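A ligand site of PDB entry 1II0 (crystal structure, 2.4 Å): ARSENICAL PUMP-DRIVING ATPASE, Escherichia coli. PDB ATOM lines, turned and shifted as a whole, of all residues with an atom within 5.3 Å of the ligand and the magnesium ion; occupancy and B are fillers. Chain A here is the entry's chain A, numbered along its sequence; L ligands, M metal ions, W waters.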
ATOM      1  N   GLN A 208       3.828  29.993  22.345  1.00  0.00           N
ATOM      2  CA  GLN A 208       4.608  29.236  23.330  1.00  0.00           C
ATOM      3  C   GLN A 208       4.411  29.865  24.709  1.00  0.00           C
ATOM      4  O   GLN A 208       4.562  31.075  24.873  1.00  0.00           O
ATOM      5  CB  GLN A 208       6.102  29.221  23.008  1.00  0.00           C
ATOM      6  CG  GLN A 208       6.895  28.637  24.168  1.00  0.00           C
ATOM      7  CD  GLN A 208       8.357  28.388  23.865  1.00  0.00           C
ATOM      8  OE1 GLN A 208       9.128  29.312  23.592  1.00  0.00           O
ATOM      9  NE2 GLN A 208       8.759  27.127  23.909  1.00  0.00           N
ATOM     10  N   SER A 210       6.182  30.042  27.340  1.00  0.00           N
ATOM     11  CA  SER A 210       7.300  30.860  27.797  1.00  0.00           C
ATOM     12  C   SER A 210       7.305  32.261  27.185  1.00  0.00           C
ATOM     13  O   SER A 210       7.468  33.254  27.885  1.00  0.00           O
ATOM     14  CB  SER A 210       8.617  30.160  27.477  1.00  0.00           C
ATOM     15  OG  SER A 210       9.732  30.956  27.851  1.00  0.00           O
ATOM     16  N   ARG A 255       0.334  21.626  21.289  1.00  0.00           N
ATOM     17  CA  ARG A 255       0.981  22.488  22.267  1.00  0.00           C
ATOM     18  C   ARG A 255       0.600  23.961  22.030  1.00  0.00           C
ATOM     19  O   ARG A 255       0.437  24.726  22.978  1.00  0.00           O
ATOM     20  CB  ARG A 255       2.498  22.296  22.194  1.00  0.00           C
ATOM     21  CG  ARG A 255       3.282  22.911  23.332  1.00  0.00           C
ATOM     22  CD  ARG A 255       4.528  22.075  23.632  1.00  0.00           C
ATOM     23  NE  ARG A 255       5.417  21.916  22.476  1.00  0.00           N
ATOM     24  CZ  ARG A 255       6.394  21.019  22.404  1.00  0.00           C
ATOM     25  NH1 ARG A 255       6.620  20.189  23.417  1.00  0.00           N
ATOM     26  NH2 ARG A 255       7.158  20.942  21.323  1.00  0.00           N
ATOM     27  N   LYS A 335      20.509  34.627  25.039  1.00  0.00           N
ATOM     28  CA  LYS A 335      19.393  35.543  25.211  1.00  0.00           C
ATOM     29  C   LYS A 335      18.272  34.849  25.972  1.00  0.00           C
ATOM     30  O   LYS A 335      18.331  33.648  26.210  1.00  0.00           O
ATOM     31  CB  LYS A 335      18.890  36.017  23.860  1.00  0.00           C
ATOM     32  CG  LYS A 335      20.005  36.535  22.955  1.00  0.00           C
ATOM     33  CD  LYS A 335      20.707  37.763  23.523  1.00  0.00           C
ATOM     34  CE  LYS A 335      19.807  38.999  23.430  1.00  0.00           C
ATOM     35  NZ  LYS A 335      20.582  40.262  23.662  1.00  0.00           N
ATOM     36  N   GLY A 336      17.261  35.622  26.358  1.00  0.00           N
ATOM     37  CA  GLY A 336      16.149  35.062  27.092  1.00  0.00           C
ATOM     38  C   GLY A 336      15.400  34.053  26.257  1.00  0.00           C
ATOM     39  O   GLY A 336      15.288  34.212  25.034  1.00  0.00           O
ATOM     40  N   GLY A 337      14.914  32.989  26.906  1.00  0.00           N
ATOM     41  CA  GLY A 337      14.142  31.954  26.224  1.00  0.00           C
ATOM     42  C   GLY A 337      14.802  30.968  25.277  1.00  0.00           C
ATOM     43  O   GLY A 337      14.124  30.087  24.765  1.00  0.00           O
ATOM     44  N   VAL A 338      16.102  31.077  25.016  1.00  0.00           N
ATOM     45  CA  VAL A 338      16.727  30.139  24.095  1.00  0.00           C
ATOM     46  C   VAL A 338      16.823  28.696  24.617  1.00  0.00           C
ATOM     47  O   VAL A 338      17.043  27.782  23.842  1.00  0.00           O
ATOM     48  CB  VAL A 338      18.110  30.615  23.681  1.00  0.00           C
ATOM     49  CG1 VAL A 338      17.996  31.966  22.984  1.00  0.00           C
ATOM     50  CG2 VAL A 338      19.019  30.708  24.911  1.00  0.00           C
ATOM     51  N   GLY A 339      16.654  28.499  25.915  1.00  0.00           N
ATOM     52  CA  GLY A 339      16.729  27.164  26.473  1.00  0.00           C
ATOM     53  C   GLY A 339      17.932  26.948  27.383  1.00  0.00           C
ATOM     54  O   GLY A 339      18.431  25.817  27.522  1.00  0.00           O
ATOM     55  N   LYS A 340      18.402  28.040  27.998  1.00  0.00           N
ATOM     56  CA  LYS A 340      19.548  27.967  28.887  1.00  0.00           C
ATOM     57  C   LYS A 340      19.297  27.012  30.028  1.00  0.00           C
ATOM     58  O   LYS A 340      20.085  26.094  30.259  1.00  0.00           O
ATOM     59  CB  LYS A 340      19.909  29.358  29.435  1.00  0.00           C
ATOM     60  CG  LYS A 340      20.542  30.292  28.399  1.00  0.00           C
ATOM     61  CD  LYS A 340      21.040  31.595  29.007  1.00  0.00           C
ATOM     62  CE  LYS A 340      19.921  32.347  29.694  1.00  0.00           C
ATOM     63  NZ  LYS A 340      18.822  32.656  28.753  1.00  0.00           N
ATOM     64  N   THR A 341      18.189  27.209  30.732  1.00  0.00           N
ATOM     65  CA  THR A 341      17.833  26.356  31.865  1.00  0.00           C
ATOM     66  C   THR A 341      17.686  24.865  31.505  1.00  0.00           C
ATOM     67  O   THR A 341      18.107  24.000  32.275  1.00  0.00           O
ATOM     68  CB  THR A 341      16.539  26.848  32.527  1.00  0.00           C
ATOM     69  OG1 THR A 341      16.764  28.147  33.091  1.00  0.00           O
ATOM     70  CG2 THR A 341      16.106  25.897  33.639  1.00  0.00           C
ATOM     71  N   THR A 342      17.112  24.575  30.342  1.00  0.00           N
ATOM     72  CA  THR A 342      16.920  23.189  29.938  1.00  0.00           C
ATOM     73  C   THR A 342      18.254  22.511  29.610  1.00  0.00           C
ATOM     74  O   THR A 342      18.476  21.357  29.965  1.00  0.00           O
ATOM     75  CB  THR A 342      15.968  23.094  28.734  1.00  0.00           C
ATOM     76  OG1 THR A 342      14.732  23.734  29.045  1.00  0.00           O
ATOM     77  CG2 THR A 342      15.678  21.638  28.430  1.00  0.00           C
ATOM     78  N   MET A 343      19.139  23.227  28.926  1.00  0.00           N
ATOM     79  CA  MET A 343      20.430  22.661  28.577  1.00  0.00           C
ATOM     80  C   MET A 343      21.208  22.475  29.870  1.00  0.00           C
ATOM     81  O   MET A 343      21.855  21.439  30.070  1.00  0.00           O
ATOM     82  CB  MET A 343      21.199  23.568  27.607  1.00  0.00           C
ATOM     83  CG  MET A 343      20.449  23.876  26.297  1.00  0.00           C
ATOM     84  SD  MET A 343      20.067  22.428  25.248  1.00  0.00           S
ATOM     85  CE  MET A 343      18.516  21.908  25.881  1.00  0.00           C
ATOM     86  N   SER A 363      17.738  29.632  38.380  1.00  0.00           N
ATOM     87  CA  SER A 363      17.045  30.833  38.815  1.00  0.00           C
ATOM     88  C   SER A 363      15.599  30.727  38.376  1.00  0.00           C
ATOM     89  O   SER A 363      14.939  31.728  38.132  1.00  0.00           O
ATOM     90  CB  SER A 363      17.716  32.054  38.198  1.00  0.00           C
ATOM     91  OG  SER A 363      17.994  31.827  36.823  1.00  0.00           O
ATOM     92  N   ASP A 364      15.109  29.489  38.288  1.00  0.00           N
ATOM     93  CA  ASP A 364      13.745  29.203  37.850  1.00  0.00           C
ATOM     94  C   ASP A 364      13.238  27.890  38.474  1.00  0.00           C
ATOM     95  O   ASP A 364      13.987  26.930  38.619  1.00  0.00           O
ATOM     96  CB  ASP A 364      13.738  29.133  36.313  1.00  0.00           C
ATOM     97  CG  ASP A 364      12.409  28.660  35.739  1.00  0.00           C
ATOM     98  OD1 ASP A 364      11.341  29.148  36.155  1.00  0.00           O
ATOM     99  OD2 ASP A 364      12.443  27.789  34.836  1.00  0.00           O
ATOM    100  N   ASP A 447      22.760  28.173  34.784  1.00  0.00           N
ATOM    101  CA  ASP A 447      21.910  28.397  33.609  1.00  0.00           C
ATOM    102  C   ASP A 447      21.751  29.840  33.175  1.00  0.00           C
ATOM    103  O   ASP A 447      20.903  30.149  32.338  1.00  0.00           O
ATOM    104  CB  ASP A 447      20.521  27.780  33.824  1.00  0.00           C
ATOM    105  CG  ASP A 447      19.681  28.528  34.834  1.00  0.00           C
ATOM    106  OD1 ASP A 447      20.245  29.319  35.631  1.00  0.00           O
ATOM    107  OD2 ASP A 447      18.453  28.326  34.839  1.00  0.00           O
ATOM    108  N   ASN A 527      19.804  24.929  20.010  1.00  0.00           N
ATOM    109  CA  ASN A 527      18.598  24.262  20.519  1.00  0.00           C
ATOM    110  C   ASN A 527      17.410  24.401  19.568  1.00  0.00           C
ATOM    111  O   ASN A 527      17.430  25.222  18.651  1.00  0.00           O
ATOM    112  CB  ASN A 527      18.263  24.851  21.897  1.00  0.00           C
ATOM    113  CG  ASN A 527      17.127  24.133  22.594  1.00  0.00           C
ATOM    114  OD1 ASN A 527      16.885  22.961  22.361  1.00  0.00           O
ATOM    115  ND2 ASN A 527      16.447  24.844  23.477  1.00  0.00           N
ATOM    116  N   ASN A 528      16.377  23.583  19.789  1.00  0.00           N
ATOM    117  CA  ASN A 528      15.174  23.600  18.953  1.00  0.00           C
ATOM    118  C   ASN A 528      15.406  23.404  17.468  1.00  0.00           C
ATOM    119  O   ASN A 528      14.914  24.174  16.649  1.00  0.00           O
ATOM    120  CB  ASN A 528      14.419  24.917  19.145  1.00  0.00           C
ATOM    121  CG  ASN A 528      13.744  25.016  20.492  1.00  0.00           C
ATOM    122  OD1 ASN A 528      12.812  24.250  20.786  1.00  0.00           O
ATOM    123  ND2 ASN A 528      14.197  25.955  21.314  1.00  0.00           N
ATOM    124  N   VAL A 565      20.521  20.189  19.200  1.00  0.00           N
ATOM    125  CA  VAL A 565      19.475  19.589  20.019  1.00  0.00           C
ATOM    126  C   VAL A 565      18.172  19.650  19.237  1.00  0.00           C
ATOM    127  O   VAL A 565      17.864  20.663  18.589  1.00  0.00           O
ATOM    128  CB  VAL A 565      19.335  20.310  21.384  1.00  0.00           C
ATOM    129  CG1 VAL A 565      18.256  19.649  22.217  1.00  0.00           C
ATOM    130  CG2 VAL A 565      20.676  20.252  22.132  1.00  0.00           C
ATOM    131  N   PRO A 566      17.377  18.571  19.261  1.00  0.00           N
ATOM    132  CA  PRO A 566      16.119  18.528  18.522  1.00  0.00           C
ATOM    133  C   PRO A 566      14.960  19.274  19.163  1.00  0.00           C
ATOM    134  O   PRO A 566      14.955  19.519  20.372  1.00  0.00           O
ATOM    135  CB  PRO A 566      15.840  17.047  18.445  1.00  0.00           C
ATOM    136  CG  PRO A 566      16.268  16.602  19.810  1.00  0.00           C
ATOM    137  CD  PRO A 566      17.608  17.291  19.963  1.00  0.00           C
ATOM    138  N   VAL A 567      13.996  19.642  18.334  1.00  0.00           N
ATOM    139  CA  VAL A 567      12.773  20.286  18.802  1.00  0.00           C
ATOM    140  C   VAL A 567      12.026  19.099  19.375  1.00  0.00           C
ATOM    141  O   VAL A 567      11.648  18.191  18.640  1.00  0.00           O
ATOM    142  CB  VAL A 567      11.930  20.851  17.635  1.00  0.00           C
ATOM    143  CG1 VAL A 567      10.638  21.427  18.175  1.00  0.00           C
ATOM    144  CG2 VAL A 567      12.708  21.915  16.889  1.00  0.00           C
ATOM    145  N   LEU A 568      11.817  19.092  20.683  1.00  0.00           N
ATOM    146  CA  LEU A 568      11.151  17.969  21.319  1.00  0.00           C
ATOM    147  C   LEU A 568       9.638  17.920  21.103  1.00  0.00           C
ATOM    148  O   LEU A 568       8.944  18.946  21.191  1.00  0.00           O
ATOM    149  CB  LEU A 568      11.461  17.942  22.823  1.00  0.00           C
ATOM    150  CG  LEU A 568      11.925  16.588  23.363  1.00  0.00           C
ATOM    151  CD1 LEU A 568      12.293  16.726  24.825  1.00  0.00           C
ATOM    152  CD2 LEU A 568      10.838  15.541  23.181  1.00  0.00           C
ATOM    153  N   SER A 570       7.702  16.866  22.991  1.00  0.00           N
ATOM    154  CA  SER A 570       7.077  17.070  24.295  1.00  0.00           C
ATOM    155  C   SER A 570       7.770  18.186  25.069  1.00  0.00           C
ATOM    156  O   SER A 570       8.690  18.832  24.569  1.00  0.00           O
ATOM    157  CB  SER A 570       7.118  15.770  25.089  1.00  0.00           C
ATOM    158  OG  SER A 570       6.263  15.862  26.216  1.00  0.00           O
ATOM    159  N   GLU A 571       7.323  18.408  26.300  1.00  0.00           N
ATOM    160  CA  GLU A 571       7.903  19.445  27.149  1.00  0.00           C
ATOM    161  C   GLU A 571       9.015  18.853  28.004  1.00  0.00           C
ATOM    162  O   GLU A 571       8.751  18.064  28.911  1.00  0.00           O
ATOM    163  CB  GLU A 571       6.830  20.053  28.051  1.00  0.00           C
ATOM    164  CG  GLU A 571       6.976  21.556  28.296  1.00  0.00           C
ATOM    165  CD  GLU A 571       6.919  22.356  26.999  1.00  0.00           C
ATOM    166  OE1 GLU A 571       6.571  23.556  27.057  1.00  0.00           O
ATOM    167  OE2 GLU A 571       7.240  21.805  25.929  1.00  0.00           O
ATOM    168  N   PRO A 572      10.276  19.215  27.724  1.00  0.00           N
ATOM    169  CA  PRO A 572      11.440  18.716  28.463  1.00  0.00           C
ATOM    170  C   PRO A 572      11.386  19.062  29.949  1.00  0.00           C
ATOM    171  O   PRO A 572      12.280  19.688  30.501  1.00  0.00           O
ATOM    172  CB  PRO A 572      12.610  19.386  27.741  1.00  0.00           C
ATOM    173  CG  PRO A 572      12.013  20.662  27.264  1.00  0.00           C
ATOM    174  CD  PRO A 572      10.691  20.226  26.724  1.00  0.00           C
ATOM    175  N   LEU A 581      16.862  14.669  24.998  1.00  0.00           N
ATOM    176  CA  LEU A 581      17.515  15.797  24.324  1.00  0.00           C
ATOM    177  C   LEU A 581      18.979  15.542  23.983  1.00  0.00           C
ATOM    178  O   LEU A 581      19.477  15.983  22.943  1.00  0.00           O
ATOM    179  CB  LEU A 581      17.450  17.040  25.214  1.00  0.00           C
ATOM    180  CG  LEU A 581      16.117  17.775  25.395  1.00  0.00           C
ATOM    181  CD1 LEU A 581      16.266  18.839  26.464  1.00  0.00           C
ATOM    182  CD2 LEU A 581      15.673  18.395  24.081  1.00  0.00           C
HETATM  183  P1  LIG L   1      14.967  32.399  30.504  1.00  0.00           P
HETATM  184  O1  LIG L   1      15.863  33.255  29.640  1.00  0.00           O
HETATM  185  O2  LIG L   1      15.516  31.970  31.819  1.00  0.00           O
HETATM  186  O3  LIG L   1      13.505  32.760  30.513  1.00  0.00           O
HETATM  187  P2  LIG L   1      15.973  29.923  29.199  1.00  0.00           P
HETATM  188  O4  LIG L   1      16.468  29.316  30.482  1.00  0.00           O
HETATM  189  O5  LIG L   1      16.881  30.552  28.197  1.00  0.00           O
HETATM  190  O6  LIG L   1      14.905  31.018  29.679  1.00  0.00           O
HETATM  191  P3  LIG L   1      14.190  27.607  29.031  1.00  0.00           P
HETATM  192  O7  LIG L   1      15.140  26.484  29.294  1.00  0.00           O
HETATM  193  O8  LIG L   1      13.329  27.984  30.216  1.00  0.00           O
HETATM  194  O9  LIG L   1      14.949  28.919  28.511  1.00  0.00           O
HETATM  195  O10 LIG L   1      13.385  27.376  27.687  1.00  0.00           O
HETATM  196  C1  LIG L   1      12.188  28.057  27.317  1.00  0.00           C
HETATM  197  C2  LIG L   1      10.993  27.133  27.108  1.00  0.00           C
HETATM  198  O11 LIG L   1      11.228  26.377  25.893  1.00  0.00           O
HETATM  199  C3  LIG L   1      10.718  26.121  28.222  1.00  0.00           C
HETATM  200  O12 LIG L   1       9.362  26.237  28.646  1.00  0.00           O
HETATM  201  C4  LIG L   1      11.156  24.761  27.679  1.00  0.00           C
HETATM  202  O13 LIG L   1      10.670  23.490  28.094  1.00  0.00           O
HETATM  203  C5  LIG L   1      11.144  24.990  26.165  1.00  0.00           C
HETATM  204  N1  LIG L   1      12.273  24.317  25.503  1.00  0.00           N
HETATM  205  C6  LIG L   1      13.634  24.554  25.644  1.00  0.00           C
HETATM  206  N2  LIG L   1      14.424  23.775  24.933  1.00  0.00           N
HETATM  207  C7  LIG L   1      13.525  22.950  24.257  1.00  0.00           C
HETATM  208  C8  LIG L   1      13.604  21.872  23.329  1.00  0.00           C
HETATM  209  N3  LIG L   1      14.744  21.369  22.855  1.00  0.00           N
HETATM  210  N4  LIG L   1      12.481  21.248  22.847  1.00  0.00           N
HETATM  211  C9  LIG L   1      11.239  21.640  23.218  1.00  0.00           C
HETATM  212  N5  LIG L   1      11.099  22.654  24.096  1.00  0.00           N
HETATM  213  C10 LIG L   1      12.204  23.287  24.589  1.00  0.00           C
HETATM  214 MG    MG M   1      16.441  30.141  32.390  1.00  0.00          MG
HETATM  215  O   HOH W   1      11.717  30.459  29.818  1.00  0.00           O
HETATM  216  O   HOH W   2      16.175  30.602  34.502  1.00  0.00           O
HETATM  217  O   HOH W   3      12.272  23.002  30.358  1.00  0.00           O
HETATM  218  O   HOH W   4      14.464  29.359  32.644  1.00  0.00           O
HETATM  219  O   HOH W   5      18.211  30.985  32.495  1.00  0.00           O
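The side-chain hydroxyl (OG1) of Thr 341 lies close to the side-chain carboxylate (OD2) of Asp 447.
ND2 of Asn 527 sits at hydrogen-bond distance from O of Val 338, at 3.0 Å.
ND2 of Asn 527 sits close to ND2 of Asn 528 (3.3 Å).
The side-chain amino group (NZ) of Lys 340 lies within hydrogen-bond range of the backbone carbonyl oxygen (O) of Lys 335 (2.8 Å).
The backbone carbonyl oxygen (O) of Leu 568 sits at hydrogen-bond distance from the guanidinium group (NH2) of Arg 255, at 2.7 Å.
O of Val 565 is in hydrogen-bond range of N of Asn 528 (3.5 Å).
The backbone NH (N) of Thr 341 lies within hydrogen-bond range of an oxygen (O7) of the ligand (3.4 Å).
The side-chain amide nitrogen of Asn 527 lies within hydrogen-bond range of a nitrogen (N2) of the ligand, 2.7 Å away.
The backbone NH (N) of Thr 342 sits at hydrogen-bond distance from an oxygen (O7) of the ligand.
An oxygen (O7) of the ligand is in hydrogen-bond range of the side-chain hydroxyl of Thr 342 (2.8 Å).
The backbone NH (N) of Gly 337 is in hydrogen-bond range of an oxygen (O1) of the ligand (2.9 Å).
N of Lys 340 is in hydrogen-bond range of O5 of the ligand, at 2.9 Å.
The side-chain amino group of Lys 340 lies within salt-bridge range of an oxygen (O5) of the ligand (2.9 Å).
N of Gly 339 lies within hydrogen-bond range of O5 of the ligand (3.1 Å).
The backbone carbonyl oxygen (O) of Pro 566 is in hydrogen-bond range of a nitrogen (N3) of the ligand (3.1 Å).
N of Leu 568 is in hydrogen-bond range of N4 of the ligand, at 3.1 Å.
NE2 of Gln 208 is in hydrogen-bond range of O11 of the ligand (3.3 Å).
The backbone NH (N) of Val 338 sits at hydrogen-bond distance from an oxygen (O5) of the ligand (3.3 Å).
Asp 447 touches the magnesium ion.
Within 4 Å of the magnesium ion: Thr 341 and Asp 447.
The nearest printed residue that does not touch the magnesium ion is Lys 340 (4.6 Å).
The magnesium ion is bound by water W5 (2.0 Å), an oxygen (O4) of the ligand (2.1 Å), an oxygen (O2) of the ligand (2.1 Å), the side-chain hydroxyl of Thr 341 (2.1 Å), water W4 (2.1 Å) and water W2 (2.2 Å).
The magnesium ion has six donor atoms within binding distance.
Water W2 lies within hydrogen-bond range of the side-chain hydroxyl (OG) of Ser 363 (3.2 Å) and the side-chain carboxylate (OD2) of Asp 447 (3.2 Å).
Water W4 lies within hydrogen-bond range of O8 of the ligand and OD2 of Asp 364.
Water W3 lies within hydrogen-bond range of O13 of the ligand (2.8 Å), OG1 of Thr 342 (2.9 Å) and O of Pro 572 (3.3 Å).
Water W1 lies within hydrogen-bond range of the side-chain hydroxyl of Ser 210 and an oxygen (O8) of the ligand.
Residues that only touch the ligand: Ser 210, Lys 335, Gly 336, Asn 528, Val 565, Pro 572 and Leu 581.
Of the 25 residues printed, 17 come within 4 Å of the ligand.
The nearest printed residue that does not touch the ligand is Ser 570 (4.03 Å).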
